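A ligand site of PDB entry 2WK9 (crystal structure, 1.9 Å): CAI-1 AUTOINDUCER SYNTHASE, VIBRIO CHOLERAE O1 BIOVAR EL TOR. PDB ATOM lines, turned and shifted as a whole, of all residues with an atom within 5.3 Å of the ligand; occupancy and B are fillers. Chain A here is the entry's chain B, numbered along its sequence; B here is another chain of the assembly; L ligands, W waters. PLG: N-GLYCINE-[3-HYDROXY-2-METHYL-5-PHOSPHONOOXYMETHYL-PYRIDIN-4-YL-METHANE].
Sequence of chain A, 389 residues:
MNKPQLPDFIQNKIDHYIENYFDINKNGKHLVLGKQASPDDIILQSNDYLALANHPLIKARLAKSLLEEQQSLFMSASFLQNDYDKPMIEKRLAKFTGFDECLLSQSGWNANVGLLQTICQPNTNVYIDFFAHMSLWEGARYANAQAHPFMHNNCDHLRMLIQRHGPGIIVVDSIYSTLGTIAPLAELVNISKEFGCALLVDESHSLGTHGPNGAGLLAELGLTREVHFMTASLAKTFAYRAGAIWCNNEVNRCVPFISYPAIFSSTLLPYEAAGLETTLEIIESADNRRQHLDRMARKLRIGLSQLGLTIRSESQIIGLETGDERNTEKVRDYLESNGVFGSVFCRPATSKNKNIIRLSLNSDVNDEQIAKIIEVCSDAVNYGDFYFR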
ATOM      1  N   ASN A  47      -1.584  10.203  30.089  1.00  0.00           N
ATOM      2  CA  ASN A  47      -1.255  11.486  29.478  1.00  0.00           C
ATOM      3  C   ASN A  47       0.062  12.047  30.012  1.00  0.00           C
ATOM      4  O   ASN A  47       0.393  13.208  29.774  1.00  0.00           O
ATOM      5  CB  ASN A  47      -2.366  12.494  29.776  1.00  0.00           C
ATOM      6  CG  ASN A  47      -3.712  12.052  29.240  1.00  0.00           C
ATOM      7  OD1 ASN A  47      -4.595  11.686  30.015  1.00  0.00           O
ATOM      8  ND2 ASN A  47      -3.868  12.102  27.931  1.00  0.00           N
ATOM      9  N   SER A 107      -8.126  21.985  38.411  1.00  0.00           N
ATOM     10  CA  SER A 107      -8.089  21.058  37.285  1.00  0.00           C
ATOM     11  C   SER A 107      -8.131  21.852  35.985  1.00  0.00           C
ATOM     12  O   SER A 107      -8.486  23.031  36.007  1.00  0.00           O
ATOM     13  CB  SER A 107      -9.260  20.080  37.325  1.00  0.00           C
ATOM     14  OG  SER A 107     -10.500  20.755  37.215  1.00  0.00           O
ATOM     15  N   GLY A 108      -7.744  21.223  34.890  1.00  0.00           N
ATOM     16  CA  GLY A 108      -7.885  21.844  33.576  1.00  0.00           C
ATOM     17  C   GLY A 108      -9.362  22.102  33.301  1.00  0.00           C
ATOM     18  O   GLY A 108      -9.707  23.115  32.706  1.00  0.00           O
ATOM     19  N   TRP A 109     -10.217  21.178  33.720  1.00  0.00           N
ATOM     20  CA  TRP A 109     -11.656  21.363  33.543  1.00  0.00           C
ATOM     21  C   TRP A 109     -12.101  22.688  34.181  1.00  0.00           C
ATOM     22  O   TRP A 109     -12.819  23.472  33.548  1.00  0.00           O
ATOM     23  CB  TRP A 109     -12.448  20.182  34.134  1.00  0.00           C
ATOM     24  CG  TRP A 109     -13.938  20.391  34.136  1.00  0.00           C
ATOM     25  CD1 TRP A 109     -14.675  21.148  35.020  1.00  0.00           C
ATOM     26  CD2 TRP A 109     -14.881  19.816  33.220  1.00  0.00           C
ATOM     27  NE1 TRP A 109     -16.002  21.084  34.705  1.00  0.00           N
ATOM     28  CE2 TRP A 109     -16.162  20.287  33.603  1.00  0.00           C
ATOM     29  CE3 TRP A 109     -14.780  18.962  32.118  1.00  0.00           C
ATOM     30  CZ2 TRP A 109     -17.318  19.927  32.919  1.00  0.00           C
ATOM     31  CZ3 TRP A 109     -15.933  18.613  31.447  1.00  0.00           C
ATOM     32  CH2 TRP A 109     -17.188  19.085  31.845  1.00  0.00           C
ATOM     33  N   ASN A 110     -11.676  22.919  35.424  1.00  0.00           N
ATOM     34  CA  ASN A 110     -12.094  24.121  36.145  1.00  0.00           C
ATOM     35  C   ASN A 110     -11.473  25.368  35.539  1.00  0.00           C
ATOM     36  O   ASN A 110     -12.062  26.456  35.588  1.00  0.00           O
ATOM     37  CB  ASN A 110     -11.719  24.048  37.636  1.00  0.00           C
ATOM     38  CG  ASN A 110     -12.548  23.050  38.405  1.00  0.00           C
ATOM     39  OD1 ASN A 110     -13.420  22.383  37.844  1.00  0.00           O
ATOM     40  ND2 ASN A 110     -12.277  22.932  39.706  1.00  0.00           N
ATOM     41  N   ASN A 112     -10.861  25.937  32.317  1.00  0.00           N
ATOM     42  CA  ASN A 112     -11.698  26.279  31.172  1.00  0.00           C
ATOM     43  C   ASN A 112     -13.065  26.819  31.555  1.00  0.00           C
ATOM     44  O   ASN A 112     -13.515  27.836  31.037  1.00  0.00           O
ATOM     45  CB  ASN A 112     -11.870  25.065  30.266  1.00  0.00           C
ATOM     46  CG  ASN A 112     -10.654  24.799  29.431  1.00  0.00           C
ATOM     47  OD1 ASN A 112      -9.831  25.680  29.242  1.00  0.00           O
ATOM     48  ND2 ASN A 112     -10.535  23.579  28.915  1.00  0.00           N
ATOM     49  N   HIS A 133     -12.223  20.332  23.575  1.00  0.00           N
ATOM     50  CA  HIS A 133     -12.536  19.566  24.784  1.00  0.00           C
ATOM     51  C   HIS A 133     -13.892  19.893  25.400  1.00  0.00           C
ATOM     52  O   HIS A 133     -14.319  21.042  25.427  1.00  0.00           O
ATOM     53  CB  HIS A 133     -11.429  19.693  25.841  1.00  0.00           C
ATOM     54  CG  HIS A 133     -11.520  18.670  26.922  1.00  0.00           C
ATOM     55  ND1 HIS A 133     -12.000  18.968  28.182  1.00  0.00           N
ATOM     56  CD2 HIS A 133     -11.237  17.351  26.936  1.00  0.00           C
ATOM     57  CE1 HIS A 133     -11.976  17.871  28.927  1.00  0.00           C
ATOM     58  NE2 HIS A 133     -11.524  16.869  28.189  1.00  0.00           N
ATOM     59  N   SER A 135     -14.857  20.333  28.233  1.00  0.00           N
ATOM     60  CA  SER A 135     -14.823  21.346  29.291  1.00  0.00           C
ATOM     61  C   SER A 135     -15.044  22.744  28.723  1.00  0.00           C
ATOM     62  O   SER A 135     -15.546  23.640  29.401  1.00  0.00           O
ATOM     63  CB  SER A 135     -13.490  21.303  30.051  1.00  0.00           C
ATOM     64  OG  SER A 135     -12.405  21.605  29.181  1.00  0.00           O
ATOM     65  N   ASP A 173      -8.413  23.632  20.815  1.00  0.00           N
ATOM     66  CA  ASP A 173      -7.300  22.913  21.427  1.00  0.00           C
ATOM     67  C   ASP A 173      -6.090  23.194  20.528  1.00  0.00           C
ATOM     68  O   ASP A 173      -6.237  23.251  19.319  1.00  0.00           O
ATOM     69  CB  ASP A 173      -7.531  21.394  21.421  1.00  0.00           C
ATOM     70  CG  ASP A 173      -8.634  20.948  22.373  1.00  0.00           C
ATOM     71  OD1 ASP A 173      -9.351  21.802  22.946  1.00  0.00           O
ATOM     72  OD2 ASP A 173      -8.792  19.715  22.545  1.00  0.00           O
ATOM     73  N   ILE A 175      -3.492  21.080  20.438  1.00  0.00           N
ATOM     74  CA  ILE A 175      -3.428  19.692  19.971  1.00  0.00           C
ATOM     75  C   ILE A 175      -4.669  18.971  20.503  1.00  0.00           C
ATOM     76  O   ILE A 175      -4.945  19.008  21.706  1.00  0.00           O
ATOM     77  CB  ILE A 175      -2.158  18.977  20.479  1.00  0.00           C
ATOM     78  CG1 ILE A 175      -0.908  19.602  19.864  1.00  0.00           C
ATOM     79  CG2 ILE A 175      -2.208  17.489  20.171  1.00  0.00           C
ATOM     80  CD1 ILE A 175       0.382  18.898  20.242  1.00  0.00           C
ATOM     81  N   SER A 177      -7.454  16.325  21.745  1.00  0.00           N
ATOM     82  CA  SER A 177      -7.290  15.259  22.738  1.00  0.00           C
ATOM     83  C   SER A 177      -7.561  13.841  22.208  1.00  0.00           C
ATOM     84  O   SER A 177      -6.923  12.891  22.661  1.00  0.00           O
ATOM     85  CB  SER A 177      -8.136  15.531  23.987  1.00  0.00           C
ATOM     86  OG  SER A 177      -9.521  15.596  23.675  1.00  0.00           O
ATOM     87  N   ASP A 202      -6.425  26.034  24.340  1.00  0.00           N
ATOM     88  CA  ASP A 202      -6.183  25.011  25.354  1.00  0.00           C
ATOM     89  C   ASP A 202      -4.951  24.187  24.953  1.00  0.00           C
ATOM     90  O   ASP A 202      -5.003  23.392  24.000  1.00  0.00           O
ATOM     91  CB  ASP A 202      -7.429  24.131  25.507  1.00  0.00           C
ATOM     92  CG  ASP A 202      -7.311  23.073  26.612  1.00  0.00           C
ATOM     93  OD1 ASP A 202      -6.186  22.621  26.908  1.00  0.00           O
ATOM     94  OD2 ASP A 202      -8.363  22.688  27.168  1.00  0.00           O
ATOM     95  N   SER A 204      -3.385  21.868  26.735  1.00  0.00           N
ATOM     96  CA  SER A 204      -3.247  20.681  27.591  1.00  0.00           C
ATOM     97  C   SER A 204      -2.328  19.618  27.014  1.00  0.00           C
ATOM     98  O   SER A 204      -1.591  18.973  27.755  1.00  0.00           O
ATOM     99  CB  SER A 204      -4.622  20.059  27.871  1.00  0.00           C
ATOM    100  OG  SER A 204      -5.406  20.893  28.710  1.00  0.00           O
ATOM    101  N   HIS A 205      -2.384  19.418  25.701  1.00  0.00           N
ATOM    102  CA  HIS A 205      -1.613  18.330  25.083  1.00  0.00           C
ATOM    103  C   HIS A 205      -0.358  18.774  24.342  1.00  0.00           C
ATOM    104  O   HIS A 205       0.289  17.963  23.688  1.00  0.00           O
ATOM    105  CB  HIS A 205      -2.522  17.477  24.195  1.00  0.00           C
ATOM    106  CG  HIS A 205      -3.675  16.874  24.938  1.00  0.00           C
ATOM    107  ND1 HIS A 205      -3.529  15.752  25.736  1.00  0.00           N
ATOM    108  CD2 HIS A 205      -4.963  17.254  25.052  1.00  0.00           C
ATOM    109  CE1 HIS A 205      -4.692  15.456  26.289  1.00  0.00           C
ATOM    110  NE2 HIS A 205      -5.585  16.355  25.894  1.00  0.00           N
ATOM    111  N   SER A 233      -4.633  21.783  31.320  1.00  0.00           N
ATOM    112  CA  SER A 233      -4.592  20.823  32.407  1.00  0.00           C
ATOM    113  C   SER A 233      -3.147  20.653  32.786  1.00  0.00           C
ATOM    114  O   SER A 233      -2.263  20.622  31.932  1.00  0.00           O
ATOM    115  CB  SER A 233      -5.112  19.457  31.956  1.00  0.00           C
ATOM    116  OG  SER A 233      -4.824  18.483  32.948  1.00  0.00           O
ATOM    117  N   LEU A 234      -2.890  20.535  34.090  1.00  0.00           N
ATOM    118  CA  LEU A 234      -1.554  20.239  34.564  1.00  0.00           C
ATOM    119  C   LEU A 234      -1.431  18.736  34.821  1.00  0.00           C
ATOM    120  O   LEU A 234      -0.424  18.260  35.351  1.00  0.00           O
ATOM    121  CB  LEU A 234      -1.269  21.051  35.824  1.00  0.00           C
ATOM    122  CG  LEU A 234      -0.420  22.319  35.708  1.00  0.00           C
ATOM    123  CD1 LEU A 234      -0.406  22.926  34.314  1.00  0.00           C
ATOM    124  CD2 LEU A 234      -0.795  23.345  36.761  1.00  0.00           C
ATOM    125  N   ALA A 235      -2.444  17.987  34.403  1.00  0.00           N
ATOM    126  CA  ALA A 235      -2.504  16.549  34.626  1.00  0.00           C
ATOM    127  C   ALA A 235      -2.001  15.735  33.437  1.00  0.00           C
ATOM    128  O   ALA A 235      -2.203  14.523  33.371  1.00  0.00           O
ATOM    129  CB  ALA A 235      -3.913  16.125  35.001  1.00  0.00           C
ATOM    130  N   LYS A 236      -1.370  16.405  32.487  1.00  0.00           N
ATOM    131  CA  LYS A 236      -0.784  15.725  31.341  1.00  0.00           C
ATOM    132  C   LYS A 236       0.740  15.673  31.538  1.00  0.00           C
ATOM    133  O   LYS A 236       1.223  14.933  32.399  1.00  0.00           O
ATOM    134  CB  LYS A 236      -1.151  16.413  30.026  1.00  0.00           C
ATOM    135  CG  LYS A 236      -2.641  16.750  29.878  1.00  0.00           C
ATOM    136  CD  LYS A 236      -3.497  15.550  30.232  1.00  0.00           C
ATOM    137  CE  LYS A 236      -4.964  15.801  29.998  1.00  0.00           C
ATOM    138  NZ  LYS A 236      -5.726  14.620  30.444  1.00  0.00           N
ATOM    139  N   ALA A 242      -4.231  19.391  38.607  1.00  0.00           N
ATOM    140  CA  ALA A 242      -4.479  20.826  38.677  1.00  0.00           C
ATOM    141  C   ALA A 242      -4.629  21.380  37.269  1.00  0.00           C
ATOM    142  O   ALA A 242      -4.513  20.655  36.283  1.00  0.00           O
ATOM    143  CB  ALA A 242      -3.339  21.531  39.411  1.00  0.00           C
ATOM    144  N   PHE A 345     -12.396   5.827  23.312  1.00  0.00           N
ATOM    145  CA  PHE A 345     -13.188   7.045  23.393  1.00  0.00           C
ATOM    146  C   PHE A 345     -14.504   6.838  22.648  1.00  0.00           C
ATOM    147  O   PHE A 345     -14.523   6.635  21.428  1.00  0.00           O
ATOM    148  CB  PHE A 345     -12.397   8.240  22.859  1.00  0.00           C
ATOM    149  CG  PHE A 345     -11.447   8.821  23.860  1.00  0.00           C
ATOM    150  CD1 PHE A 345     -10.200   8.264  24.062  1.00  0.00           C
ATOM    151  CD2 PHE A 345     -11.809   9.927  24.634  1.00  0.00           C
ATOM    152  CE1 PHE A 345      -9.329   8.779  25.007  1.00  0.00           C
ATOM    153  CE2 PHE A 345     -10.943  10.452  25.564  1.00  0.00           C
ATOM    154  CZ  PHE A 345      -9.698   9.883  25.753  1.00  0.00           C
ATOM    155  N   ARG A 358      -7.650   5.558  21.316  1.00  0.00           N
ATOM    156  CA  ARG A 358      -6.548   6.492  21.376  1.00  0.00           C
ATOM    157  C   ARG A 358      -5.286   5.849  21.910  1.00  0.00           C
ATOM    158  O   ARG A 358      -5.285   5.217  22.974  1.00  0.00           O
ATOM    159  CB  ARG A 358      -6.914   7.723  22.221  1.00  0.00           C
ATOM    160  CG  ARG A 358      -5.784   8.758  22.282  1.00  0.00           C
ATOM    161  CD  ARG A 358      -6.134   9.952  23.162  1.00  0.00           C
ATOM    162  NE  ARG A 358      -6.081   9.630  24.591  1.00  0.00           N
ATOM    163  CZ  ARG A 358      -6.360  10.491  25.561  1.00  0.00           C
ATOM    164  NH1 ARG A 358      -6.720  11.736  25.257  1.00  0.00           N
ATOM    165  NH2 ARG A 358      -6.287  10.116  26.828  1.00  0.00           N
ATOM    166  N   MET B  75      -5.355   9.941  33.752  1.00  0.00           N
ATOM    167  CA  MET B  75      -6.426   9.615  32.848  1.00  0.00           C
ATOM    168  C   MET B  75      -7.723   9.754  33.618  1.00  0.00           C
ATOM    169  O   MET B  75      -7.713   9.986  34.830  1.00  0.00           O
ATOM    170  CB  MET B  75      -6.268   8.176  32.347  1.00  0.00           C
ATOM    171  CG  MET B  75      -6.463   7.133  33.447  1.00  0.00           C
ATOM    172  SD  MET B  75      -5.683   5.535  33.115  1.00  0.00           S
ATOM    173  CE  MET B  75      -6.679   4.917  31.770  1.00  0.00           C
ATOM    174  N   SER B  76      -8.841   9.613  32.908  1.00  0.00           N
ATOM    175  CA  SER B  76     -10.157   9.681  33.542  1.00  0.00           C
ATOM    176  C   SER B  76     -10.394   8.494  34.474  1.00  0.00           C
ATOM    177  O   SER B  76      -9.888   7.391  34.234  1.00  0.00           O
ATOM    178  CB  SER B  76     -11.234   9.724  32.457  1.00  0.00           C
ATOM    179  OG  SER B  76     -12.500   9.352  32.975  1.00  0.00           O
ATOM    180  N   PHE B 264     -14.438  13.609  32.094  1.00  0.00           N
ATOM    181  CA  PHE B 264     -13.547  14.499  31.347  1.00  0.00           C
ATOM    182  C   PHE B 264     -12.473  15.210  32.170  1.00  0.00           C
ATOM    183  O   PHE B 264     -11.708  16.002  31.622  1.00  0.00           O
ATOM    184  CB  PHE B 264     -14.377  15.510  30.549  1.00  0.00           C
ATOM    185  CG  PHE B 264     -15.245  14.896  29.495  1.00  0.00           C
ATOM    186  CD1 PHE B 264     -14.709  14.482  28.288  1.00  0.00           C
ATOM    187  CD2 PHE B 264     -16.597  14.731  29.711  1.00  0.00           C
ATOM    188  CE1 PHE B 264     -15.508  13.914  27.308  1.00  0.00           C
ATOM    189  CE2 PHE B 264     -17.410  14.164  28.734  1.00  0.00           C
ATOM    190  CZ  PHE B 264     -16.866  13.760  27.532  1.00  0.00           C
ATOM    191  N   SER B 265     -12.403  14.916  33.453  1.00  0.00           N
ATOM    192  CA  SER B 265     -11.360  15.487  34.301  1.00  0.00           C
ATOM    193  C   SER B 265     -10.609  14.359  35.011  1.00  0.00           C
ATOM    194  O   SER B 265     -11.196  13.334  35.365  1.00  0.00           O
ATOM    195  CB  SER B 265     -11.962  16.476  35.288  1.00  0.00           C
ATOM    196  OG  SER B 265     -10.957  17.204  35.972  1.00  0.00           O
ATOM    197  N   SER B 266      -9.307  14.565  35.219  1.00  0.00           N
ATOM    198  CA  SER B 266      -8.431  13.515  35.754  1.00  0.00           C
ATOM    199  C   SER B 266      -8.799  13.054  37.157  1.00  0.00           C
ATOM    200  O   SER B 266      -9.323  13.819  37.960  1.00  0.00           O
ATOM    201  CB  SER B 266      -6.981  13.977  35.731  1.00  0.00           C
ATOM    202  OG  SER B 266      -6.591  14.335  34.419  1.00  0.00           O
HETATM  203  N1  PLG L   1      -8.548  20.342  28.150  1.00  0.00           N
HETATM  204  C2  PLG L   1      -8.217  19.304  27.364  1.00  0.00           C
HETATM  205  C2A PLG L   1      -7.804  19.542  25.909  1.00  0.00           C
HETATM  206  C3  PLG L   1      -8.245  17.998  27.868  1.00  0.00           C
HETATM  207  O3  PLG L   1      -7.913  16.959  27.059  1.00  0.00           O
HETATM  208  C4  PLG L   1      -8.619  17.771  29.180  1.00  0.00           C
HETATM  209  C4A PLG L   1      -8.701  16.373  29.821  1.00  0.00           C
HETATM  210  C5  PLG L   1      -8.954  18.876  29.947  1.00  0.00           C
HETATM  211  C6  PLG L   1      -8.905  20.151  29.412  1.00  0.00           C
HETATM  212  C5A PLG L   1      -9.381  18.659  31.403  1.00  0.00           C
HETATM  213  OP4 PLG L   1      -8.198  18.557  32.205  1.00  0.00           O
HETATM  214  P   PLG L   1      -8.260  18.091  33.760  1.00  0.00           P
HETATM  215  OP1 PLG L   1      -8.270  16.478  33.649  1.00  0.00           O
HETATM  216  OP2 PLG L   1      -9.659  18.548  34.376  1.00  0.00           O
HETATM  217  OP3 PLG L   1      -7.085  18.577  34.517  1.00  0.00           O
HETATM  218  C   PLG L   1      -7.650  13.038  28.466  1.00  0.00           C
HETATM  219  O   PLG L   1      -7.204  13.537  27.414  1.00  0.00           O
HETATM  220  OXT PLG L   1      -7.606  11.839  28.784  1.00  0.00           O
HETATM  221  CA  PLG L   1      -8.293  14.006  29.465  1.00  0.00           C
HETATM  222  N   PLG L   1      -8.137  15.361  28.918  1.00  0.00           N
HETATM  223  O   HOH W   1      -6.651  17.705  36.954  1.00  0.00           O
HETATM  224  O   HOH W   2      -9.151  13.460  32.240  1.00  0.00           O
HETATM  225  O   HOH W   3     -11.092  13.973  28.270  1.00  0.00           O
HETATM  226  O   HOH W   4      -8.182   9.640  30.068  1.00  0.00           O
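CB of Ser 107 touches OP2 of the ligand (3.3 Å).
ND2 of Asn 112 touches C6 of the ligand (3.8 Å).
NE2 of His 133 touches C4 of the ligand, 3.2 Å away.
Ser 135 touches the ligand.
Asp 173 touches the ligand (OD2 to C2A, 3.5 Å).
Ser 177 touches the ligand (CB to O3, 3.4 Å).
Ala 242 touches the ligand (O to OP3, 3.7 Å).
Phe 264 of chain B touches the ligand (O to C4A, 3.5 Å).
Hydrophobic or aromatic side chains that line the ligand: Trp 109, His 133 and His 205.
Of the 26 residues printed, 19 come within 4 Å of the ligand.
OD2 of Asp 202 is in hydrogen-bond range of ND2 of Asn 112, at 2.9 Å.
The backbone NH (N) of Ser 233 sits at hydrogen-bond distance from the side-chain hydroxyl (OG) of Ser 204 (2.9 Å).
NZ of Lys 236 sits at hydrogen-bond distance from OD1 of Asn 47.
The guanidinium group of Arg 358 lies close to the side-chain amide nitrogen of Asn 47 (3.3 Å).
O of Ser 177 is in hydrogen-bond range of NH1 of Arg 358 (2.8 Å).
The backbone NH (N) of His 133 lies within hydrogen-bond range of the side-chain carboxylate (OD1) of Asp 173 (3.3 Å).
The backbone carbonyl oxygen of Ala 242 sits at hydrogen-bond distance from the backbone NH of Leu 234, 2.7 Å away.
OG of Ser 135 is in hydrogen-bond range of ND2 of Asn 112, at 2.7 Å.
OG of Ser 265 of chain B sits at hydrogen-bond distance from OP2 of the ligand (2.5 Å).
A nitrogen (N1) of the ligand lies within hydrogen-bond range of the side-chain carboxylate of Asp 202 (2.5 Å).
An oxygen (O3) of the ligand is in hydrogen-bond range of a ring nitrogen (NE2) of His 205 (2.7 Å).
N of Ser 266 of chain B is in hydrogen-bond range of OP1 of the ligand, at 2.7 Å.
The side-chain hydroxyl of Ser 266 of chain B lies within hydrogen-bond range of an oxygen (OP1) of the ligand.
The backbone NH of Gly 108 is in hydrogen-bond range of an oxygen (OP3) of the ligand.
OG of Ser 233 sits at hydrogen-bond distance from OP3 of the ligand.
The backbone NH of Trp 109 is in hydrogen-bond range of an oxygen (OP2) of the ligand, at 2.8 Å.
The side-chain amino group of Lys 236 is in salt-bridge range of an oxygen (O) of the ligand (3.5 Å).
O of the ligand lies within salt-bridge range of NH1 of Arg 358 (2.9 Å).
OG of Ser 204 is in hydrogen-bond range of N1 of the ligand, at 3.2 Å.
OD1 of Asn 47 sits close to OXT of the ligand (3.3 Å).
Water W4 bridges OXT of the ligand (2.6 Å) and N of Ser 76 of chain B (2.9 Å).
Water W1 bridges an oxygen (OP3) of the ligand (2.6 Å) and the backbone NH of Ala 242 (3.4 Å).
Water W2 lies within hydrogen-bond range of the backbone NH of Ser 266 of chain B (3.2 Å) and an oxygen (OP1) of the ligand (3.4 Å).
Water W3 bridges NE2 of His 133 (2.9 Å) and N of the ligand (3.3 Å).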
